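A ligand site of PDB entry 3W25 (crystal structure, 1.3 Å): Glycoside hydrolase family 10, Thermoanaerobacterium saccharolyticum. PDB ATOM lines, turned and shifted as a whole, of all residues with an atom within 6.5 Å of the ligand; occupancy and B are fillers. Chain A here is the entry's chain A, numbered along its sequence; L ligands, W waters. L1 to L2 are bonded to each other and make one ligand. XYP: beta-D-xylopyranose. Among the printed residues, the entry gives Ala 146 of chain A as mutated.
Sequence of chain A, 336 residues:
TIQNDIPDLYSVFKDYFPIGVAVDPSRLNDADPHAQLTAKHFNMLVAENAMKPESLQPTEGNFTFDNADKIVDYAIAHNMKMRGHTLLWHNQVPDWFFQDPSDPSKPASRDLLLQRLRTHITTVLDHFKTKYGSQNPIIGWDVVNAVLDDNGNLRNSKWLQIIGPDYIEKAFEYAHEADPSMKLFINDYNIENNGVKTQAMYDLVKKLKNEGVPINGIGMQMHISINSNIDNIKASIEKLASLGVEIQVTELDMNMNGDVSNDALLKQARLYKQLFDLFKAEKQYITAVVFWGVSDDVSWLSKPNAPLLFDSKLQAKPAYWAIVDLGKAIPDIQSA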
ATOM      1  N   GLU A  48      16.356 -14.921  37.111  1.00  0.00           N
ATOM      2  CA  GLU A  48      15.710 -14.867  35.814  1.00  0.00           C
ATOM      3  C   GLU A  48      14.984 -13.535  35.636  1.00  0.00           C
ATOM      4  O   GLU A  48      14.944 -13.014  34.509  1.00  0.00           O
ATOM      5  CB  GLU A  48      14.739 -16.046  35.713  1.00  0.00           C
ATOM      6  CG  GLU A  48      14.203 -16.235  34.280  1.00  0.00           C
ATOM      7  CD  GLU A  48      13.211 -17.416  34.130  1.00  0.00           C
ATOM      8  OE1 GLU A  48      12.864 -18.017  35.158  1.00  0.00           O
ATOM      9  OE2 GLU A  48      12.801 -17.668  32.991  1.00  0.00           O
ATOM     10  N   ASN A  49      14.391 -13.021  36.704  1.00  0.00           N
ATOM     11  CA  ASN A  49      13.623 -11.774  36.645  1.00  0.00           C
ATOM     12  C   ASN A  49      13.776 -10.854  37.836  1.00  0.00           C
ATOM     13  O   ASN A  49      13.570  -9.659  37.673  1.00  0.00           O
ATOM     14  CB  ASN A  49      12.099 -12.069  36.543  1.00  0.00           C
ATOM     15  CG  ASN A  49      11.755 -12.682  35.214  1.00  0.00           C
ATOM     16  OD1 ASN A  49      11.876 -12.010  34.156  1.00  0.00           O
ATOM     17  ND2 ASN A  49      11.360 -13.949  35.208  1.00  0.00           N
ATOM     18  N   LYS A  52      15.806  -7.433  37.442  1.00  0.00           N
ATOM     19  CA  LYS A  52      15.510  -6.524  36.360  1.00  0.00           C
ATOM     20  C   LYS A  52      15.057  -5.156  36.923  1.00  0.00           C
ATOM     21  O   LYS A  52      14.572  -5.075  38.050  1.00  0.00           O
ATOM     22  CB  LYS A  52      14.510  -7.139  35.399  1.00  0.00           C
ATOM     23  CG  LYS A  52      15.143  -8.257  34.628  1.00  0.00           C
ATOM     24  CD  LYS A  52      14.132  -9.087  33.839  1.00  0.00           C
ATOM     25  CE  LYS A  52      14.858 -10.106  32.975  1.00  0.00           C
ATOM     26  NZ  LYS A  52      13.898 -11.118  32.355  1.00  0.00           N
ATOM     27  N   HIS A  85      21.663  -9.735  36.717  1.00  0.00           N
ATOM     28  CA  HIS A  85      20.927  -9.493  35.438  1.00  0.00           C
ATOM     29  C   HIS A  85      19.712  -8.686  35.795  1.00  0.00           C
ATOM     30  O   HIS A  85      18.861  -9.181  36.534  1.00  0.00           O
ATOM     31  CB  HIS A  85      20.560 -10.857  34.861  1.00  0.00           C
ATOM     32  CG  HIS A  85      19.796 -10.756  33.538  1.00  0.00           C
ATOM     33  ND1 HIS A  85      20.438 -10.441  32.354  1.00  0.00           N
ATOM     34  CD2 HIS A  85      18.470 -10.883  33.258  1.00  0.00           C
ATOM     35  CE1 HIS A  85      19.503 -10.414  31.368  1.00  0.00           C
ATOM     36  NE2 HIS A  85      18.334 -10.653  31.896  1.00  0.00           N
ATOM     37  N   THR A  86      19.534  -7.433  35.369  1.00  0.00           N
ATOM     38  CA  THR A  86      20.426  -6.637  34.513  1.00  0.00           C
ATOM     39  C   THR A  86      20.110  -5.153  34.870  1.00  0.00           C
ATOM     40  O   THR A  86      19.000  -4.828  35.247  1.00  0.00           O
ATOM     41  CB  THR A  86      20.144  -6.921  33.002  1.00  0.00           C
ATOM     42  OG1 THR A  86      20.903  -6.017  32.155  1.00  0.00           O
ATOM     43  CG2 THR A  86      18.684  -6.751  32.590  1.00  0.00           C
ATOM     44  N   TRP A  89      17.732  -2.418  30.222  1.00  0.00           N
ATOM     45  CA  TRP A  89      17.138  -3.216  29.139  1.00  0.00           C
ATOM     46  C   TRP A  89      15.958  -2.374  28.640  1.00  0.00           C
ATOM     47  O   TRP A  89      15.564  -1.403  29.301  1.00  0.00           O
ATOM     48  CB  TRP A  89      16.638  -4.571  29.765  1.00  0.00           C
ATOM     49  CG  TRP A  89      16.242  -5.632  28.757  1.00  0.00           C
ATOM     50  CD1 TRP A  89      16.658  -5.787  27.466  1.00  0.00           C
ATOM     51  CD2 TRP A  89      15.368  -6.722  29.050  1.00  0.00           C
ATOM     52  NE1 TRP A  89      16.074  -6.953  26.934  1.00  0.00           N
ATOM     53  CE2 TRP A  89      15.267  -7.514  27.891  1.00  0.00           C
ATOM     54  CE3 TRP A  89      14.634  -7.112  30.213  1.00  0.00           C
ATOM     55  CZ2 TRP A  89      14.462  -8.660  27.810  1.00  0.00           C
ATOM     56  CZ3 TRP A  89      13.839  -8.267  30.141  1.00  0.00           C
ATOM     57  CH2 TRP A  89      13.778  -9.012  28.936  1.00  0.00           C
ATOM     58  N   GLN A  92      10.864  -4.926  30.708  1.00  0.00           N
ATOM     59  CA  GLN A  92      10.812  -5.033  32.158  1.00  0.00           C
ATOM     60  C   GLN A  92      11.524  -3.863  32.823  1.00  0.00           C
ATOM     61  O   GLN A  92      12.273  -4.033  33.817  1.00  0.00           O
ATOM     62  CB  GLN A  92      11.327  -6.393  32.636  1.00  0.00           C
ATOM     63  CG  GLN A  92      10.299  -7.521  32.190  1.00  0.00           C
ATOM     64  CD  GLN A  92      10.858  -8.877  32.537  1.00  0.00           C
ATOM     65  OE1 GLN A  92      11.442  -9.543  31.686  1.00  0.00           O
ATOM     66  NE2 GLN A  92      10.609  -9.332  33.778  1.00  0.00           N
ATOM     67  N   ASP A 142      25.333  -7.761  34.030  1.00  0.00           N
ATOM     68  CA  ASP A 142      24.949  -7.367  32.647  1.00  0.00           C
ATOM     69  C   ASP A 142      24.528  -5.895  32.847  1.00  0.00           C
ATOM     70  O   ASP A 142      23.422  -5.591  33.346  1.00  0.00           O
ATOM     71  CB  ASP A 142      23.758  -8.218  32.199  1.00  0.00           C
ATOM     72  CG  ASP A 142      24.161  -9.652  31.878  1.00  0.00           C
ATOM     73  OD1 ASP A 142      25.312  -9.871  31.477  1.00  0.00           O
ATOM     74  OD2 ASP A 142      23.241 -10.506  32.128  1.00  0.00           O
ATOM     75  N   ASN A 145      21.710  -4.688  28.395  1.00  0.00           N
ATOM     76  CA  ASN A 145      21.177  -5.947  27.810  1.00  0.00           C
ATOM     77  C   ASN A 145      20.494  -5.659  26.489  1.00  0.00           C
ATOM     78  O   ASN A 145      19.654  -4.741  26.414  1.00  0.00           O
ATOM     79  CB  ASN A 145      20.129  -6.513  28.823  1.00  0.00           C
ATOM     80  CG  ASN A 145      19.836  -7.940  28.559  1.00  0.00           C
ATOM     81  OD1 ASN A 145      20.720  -8.739  28.283  1.00  0.00           O
ATOM     82  ND2 ASN A 145      18.555  -8.330  28.705  1.00  0.00           N
ATOM     83  N   ALA A 146      20.846  -6.396  25.475  1.00  0.00           N
ATOM     84  CA  ALA A 146      20.138  -6.336  24.163  1.00  0.00           C
ATOM     85  C   ALA A 146      20.072  -4.992  23.558  1.00  0.00           C
ATOM     86  O   ALA A 146      19.001  -4.577  23.050  1.00  0.00           O
ATOM     87  CB  ALA A 146      18.721  -7.030  24.309  1.00  0.00           C
ATOM     88  N   ASN A 187      25.487  -7.696  27.275  1.00  0.00           N
ATOM     89  CA  ASN A 187      24.915  -9.024  27.028  1.00  0.00           C
ATOM     90  C   ASN A 187      23.962  -8.956  25.830  1.00  0.00           C
ATOM     91  O   ASN A 187      23.182  -7.987  25.667  1.00  0.00           O
ATOM     92  CB  ASN A 187      24.112  -9.393  28.315  1.00  0.00           C
ATOM     93  CG  ASN A 187      23.613 -10.847  28.336  1.00  0.00           C
ATOM     94  OD1 ASN A 187      24.378 -11.754  28.072  1.00  0.00           O
ATOM     95  ND2 ASN A 187      22.341 -11.041  28.704  1.00  0.00           N
ATOM     96  N   ASP A 188      23.984 -10.020  24.977  1.00  0.00           N
ATOM     97  CA  ASP A 188      23.034  -9.966  23.835  1.00  0.00           C
ATOM     98  C   ASP A 188      22.867 -11.334  23.233  1.00  0.00           C
ATOM     99  O   ASP A 188      23.672 -12.284  23.436  1.00  0.00           O
ATOM    100  CB  ASP A 188      23.553  -9.015  22.723  1.00  0.00           C
ATOM    101  CG  ASP A 188      22.407  -8.189  22.094  1.00  0.00           C
ATOM    102  OD1 ASP A 188      21.314  -8.761  22.016  1.00  0.00           O
ATOM    103  OD2 ASP A 188      22.633  -7.022  21.719  1.00  0.00           O
ATOM    104  N   TYR A 189      21.765 -11.452  22.473  1.00  0.00           N
ATOM    105  CA  TYR A 189      21.419 -12.696  21.749  1.00  0.00           C
ATOM    106  C   TYR A 189      21.705 -12.524  20.298  1.00  0.00           C
ATOM    107  O   TYR A 189      21.866 -11.437  19.771  1.00  0.00           O
ATOM    108  CB  TYR A 189      19.924 -13.028  21.966  1.00  0.00           C
ATOM    109  CG  TYR A 189      18.942 -12.002  21.470  1.00  0.00           C
ATOM    110  CD1 TYR A 189      18.334 -12.106  20.222  1.00  0.00           C
ATOM    111  CD2 TYR A 189      18.561 -10.889  22.287  1.00  0.00           C
ATOM    112  CE1 TYR A 189      17.376 -11.197  19.780  1.00  0.00           C
ATOM    113  CE2 TYR A 189      17.641  -9.955  21.821  1.00  0.00           C
ATOM    114  CZ  TYR A 189      17.064 -10.155  20.586  1.00  0.00           C
ATOM    115  OH  TYR A 189      16.116  -9.220  20.226  1.00  0.00           O
ATOM    116  N   GLN A 221      24.144 -14.524  25.148  1.00  0.00           N
ATOM    117  CA  GLN A 221      22.936 -15.191  25.685  1.00  0.00           C
ATOM    118  C   GLN A 221      22.819 -16.664  25.241  1.00  0.00           C
ATOM    119  O   GLN A 221      22.469 -17.521  26.048  1.00  0.00           O
ATOM    120  CB  GLN A 221      21.666 -14.402  25.319  1.00  0.00           C
ATOM    121  CG  GLN A 221      21.587 -13.088  26.052  1.00  0.00           C
ATOM    122  CD  GLN A 221      20.334 -12.310  25.770  1.00  0.00           C
ATOM    123  OE1 GLN A 221      20.275 -11.054  26.185  1.00  0.00           O
ATOM    124  NE2 GLN A 221      19.356 -12.891  25.200  1.00  0.00           N
ATOM    125  N   HIS A 223      20.699 -18.116  23.207  1.00  0.00           N
ATOM    126  CA  HIS A 223      19.378 -18.750  23.021  1.00  0.00           C
ATOM    127  C   HIS A 223      19.444 -19.360  21.620  1.00  0.00           C
ATOM    128  O   HIS A 223      18.992 -18.766  20.646  1.00  0.00           O
ATOM    129  CB  HIS A 223      18.334 -17.658  23.109  1.00  0.00           C
ATOM    130  CG  HIS A 223      18.107 -17.167  24.491  1.00  0.00           C
ATOM    131  ND1 HIS A 223      17.647 -18.009  25.475  1.00  0.00           N
ATOM    132  CD2 HIS A 223      18.305 -15.952  25.093  1.00  0.00           C
ATOM    133  CE1 HIS A 223      17.593 -17.370  26.638  1.00  0.00           C
ATOM    134  NE2 HIS A 223      17.969 -16.127  26.424  1.00  0.00           N
ATOM    135  N   GLU A 251      22.710 -17.325  28.929  1.00  0.00           N
ATOM    136  CA  GLU A 251      21.279 -17.671  28.972  1.00  0.00           C
ATOM    137  C   GLU A 251      20.994 -18.865  28.044  1.00  0.00           C
ATOM    138  O   GLU A 251      20.035 -18.886  27.262  1.00  0.00           O
ATOM    139  CB  GLU A 251      20.399 -16.473  28.521  1.00  0.00           C
ATOM    140  CG  GLU A 251      20.736 -15.125  29.215  1.00  0.00           C
ATOM    141  CD  GLU A 251      19.771 -14.027  28.880  1.00  0.00           C
ATOM    142  OE1 GLU A 251      18.714 -14.294  28.264  1.00  0.00           O
ATOM    143  OE2 GLU A 251      20.076 -12.875  29.265  1.00  0.00           O
ATOM    144  N   TRP A 292      19.420 -20.973  30.975  1.00  0.00           N
ATOM    145  CA  TRP A 292      18.274 -20.092  31.266  1.00  0.00           C
ATOM    146  C   TRP A 292      17.075 -20.887  31.717  1.00  0.00           C
ATOM    147  O   TRP A 292      16.053 -21.045  31.001  1.00  0.00           O
ATOM    148  CB  TRP A 292      17.974 -19.214  30.035  1.00  0.00           C
ATOM    149  CG  TRP A 292      17.288 -17.938  30.459  1.00  0.00           C
ATOM    150  CD1 TRP A 292      15.997 -17.543  30.164  1.00  0.00           C
ATOM    151  CD2 TRP A 292      17.857 -16.880  31.256  1.00  0.00           C
ATOM    152  NE1 TRP A 292      15.753 -16.265  30.738  1.00  0.00           N
ATOM    153  CE2 TRP A 292      16.878 -15.883  31.411  1.00  0.00           C
ATOM    154  CE3 TRP A 292      19.121 -16.699  31.870  1.00  0.00           C
ATOM    155  CZ2 TRP A 292      17.156 -14.691  32.178  1.00  0.00           C
ATOM    156  CZ3 TRP A 292      19.367 -15.538  32.595  1.00  0.00           C
ATOM    157  CH2 TRP A 292      18.395 -14.569  32.746  1.00  0.00           C
ATOM    158  N   SER A 299      10.881 -23.460  31.637  1.00  0.00           N
ATOM    159  CA  SER A 299      11.499 -22.628  30.620  1.00  0.00           C
ATOM    160  C   SER A 299      10.541 -21.543  30.171  1.00  0.00           C
ATOM    161  O   SER A 299       9.341 -21.733  30.070  1.00  0.00           O
ATOM    162  CB  SER A 299      11.816 -23.491  29.408  1.00  0.00           C
ATOM    163  OG  SER A 299      12.260 -22.684  28.285  1.00  0.00           O
ATOM    164  N   TRP A 300      11.147 -20.389  29.841  1.00  0.00           N
ATOM    165  CA  TRP A 300      10.389 -19.256  29.331  1.00  0.00           C
ATOM    166  C   TRP A 300       9.903 -19.463  27.925  1.00  0.00           C
ATOM    167  O   TRP A 300       9.038 -18.683  27.484  1.00  0.00           O
ATOM    168  CB  TRP A 300      11.278 -17.962  29.353  1.00  0.00           C
ATOM    169  CG  TRP A 300      12.380 -17.932  28.329  1.00  0.00           C
ATOM    170  CD1 TRP A 300      13.410 -18.816  28.164  1.00  0.00           C
ATOM    171  CD2 TRP A 300      12.540 -16.956  27.294  1.00  0.00           C
ATOM    172  NE1 TRP A 300      14.177 -18.467  27.101  1.00  0.00           N
ATOM    173  CE2 TRP A 300      13.664 -17.309  26.551  1.00  0.00           C
ATOM    174  CE3 TRP A 300      11.803 -15.800  26.925  1.00  0.00           C
ATOM    175  CZ2 TRP A 300      14.128 -16.574  25.474  1.00  0.00           C
ATOM    176  CZ3 TRP A 300      12.208 -15.064  25.847  1.00  0.00           C
ATOM    177  CH2 TRP A 300      13.362 -15.447  25.125  1.00  0.00           C
HETATM  178  O1  XYP L   1      17.032 -11.583  25.812  1.00  0.00           O
HETATM  179  C1  XYP L   1      16.733 -12.392  26.946  1.00  0.00           C
HETATM  180  C2  XYP L   1      16.768 -11.504  28.177  1.00  0.00           C
HETATM  181  C3  XYP L   1      16.170 -12.245  29.368  1.00  0.00           C
HETATM  182  C4  XYP L   1      14.794 -12.765  28.998  1.00  0.00           C
HETATM  183  C5  XYP L   1      14.934 -13.665  27.775  1.00  0.00           C
HETATM  184  O2  XYP L   1      18.133 -11.124  28.454  1.00  0.00           O
HETATM  185  O3  XYP L   1      16.045 -11.358  30.498  1.00  0.00           O
HETATM  186  O4  XYP L   1      14.265 -13.468  30.140  1.00  0.00           O
HETATM  187  O5  XYP L   1      15.405 -12.856  26.685  1.00  0.00           O
HETATM  188  C1  XYP L   2      12.840 -13.610  30.069  1.00  0.00           C
HETATM  189  C2  XYP L   2      12.434 -14.433  31.278  1.00  0.00           C
HETATM  190  C3  XYP L   2      10.929 -14.503  31.391  1.00  0.00           C
HETATM  191  C4  XYP L   2      10.354 -13.097  31.350  1.00  0.00           C
HETATM  192  C5  XYP L   2      10.858 -12.381  30.104  1.00  0.00           C
HETATM  193  O2  XYP L   2      12.982 -15.735  31.070  1.00  0.00           O
HETATM  194  O3  XYP L   2      10.573 -15.127  32.628  1.00  0.00           O
HETATM  195  O4  XYP L   2       8.911 -13.166  31.295  1.00  0.00           O
HETATM  196  O5  XYP L   2      12.283 -12.301  30.190  1.00  0.00           O
HETATM  197  O   HOH W   1       8.757 -17.095  31.983  1.00  0.00           O
HETATM  198  O   HOH W   2       7.931 -14.359  28.985  1.00  0.00           O
HETATM  199  O   HOH W   3       7.751 -10.554  31.430  1.00  0.00           O
HETATM  200  O   HOH W   4       7.945 -13.726  33.836  1.00  0.00           O
HETATM  201  O   HOH W   5      16.157  -8.878  24.851  1.00  0.00           O
HETATM  202  O   HOH W   6      13.312 -11.284  25.721  1.00  0.00           O
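O2 of XYP L2 lies within hydrogen-bond range of OE2 of Glu 48 (2.7 Å). The side-chain amide nitrogen of Gln 221 sits at hydrogen-bond distance from an oxygen (O1) of XYP L1, 2.7 Å away. The side-chain carboxylate (OE2) of Glu 251 lies within hydrogen-bond range of an oxygen (O2) of XYP L1 (2.7 Å). O3 of XYP L1 sits at hydrogen-bond distance from NE2 of His 85 (2.8 Å). The side-chain amide nitrogen of Asn 145 is in hydrogen-bond range of an oxygen (O2) of XYP L1. NE1 of Trp 292 sits at hydrogen-bond distance from O2 of XYP L2 (2.8 Å). The side-chain amino group (NZ) of Lys 52 lies within hydrogen-bond range of an oxygen (O3) of XYP L1 (2.8 Å). The side-chain amide nitrogen of Asn 49 lies within hydrogen-bond range of an oxygen (O3) of XYP L2, at 2.9 Å. OE1 of Gln 92 lies close to O5 of XYP L2, 3.2 Å away.
The backbone carbonyl oxygen (O) of Glu 48 is in hydrogen-bond range of the side-chain amino group (NZ) of Lys 52 (3.1 Å). The backbone carbonyl oxygen (O) of Gln 221 sits close to the backbone NH (N) of Glu 251, 2.9 Å away. NE2 of His 223 lies within hydrogen-bond range of OE1 of Glu 251. The side-chain amide nitrogen (ND2) of Asn 145 lies close to the indole nitrogen (NE1) of Trp 89 (3.3 Å). The side-chain amide nitrogen (ND2) of Asn 187 lies within hydrogen-bond range of the side-chain amide oxygen (OD1) of Asn 145. The side-chain amino group of Lys 52 is in hydrogen-bond range of the side-chain amide oxygen of Asn 49 (2.9 Å). The side-chain amino group of Lys 52 sits at hydrogen-bond distance from the side-chain amide oxygen of Gln 92 (3.0 Å). The side-chain amide oxygen (OD1) of Asn 49 is in hydrogen-bond range of the side-chain amide nitrogen (NE2) of Gln 92 (3.0 Å).
CH2 of Trp 89 touches O3 of XYP L1 (3.6 Å). CD2 of Tyr 189 touches O1 of XYP L1 (3.9 Å). His 223 touches the ligand. CB of Trp 300 touches O2 of XYP L2, at 3.3 Å. 13 residues have an atom within 4 Å of the ligand: Glu 48, Asn 49, Lys 52, His 85, Trp 89, Gln 92, Asn 145, Tyr 189, Gln 221, His 223, Glu 251, Trp 292 and Trp 300. Along chain A the residues within 4 Å of the ligand span positions 48 to 300. The nearest printed residue that does not touch the ligand is Asn 187 (4.2 Å).
Water W5 bridges the indole nitrogen (NE1) of Trp 89 (2.8 Å) and an oxygen (O1) of XYP L1 (3.0 Å).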
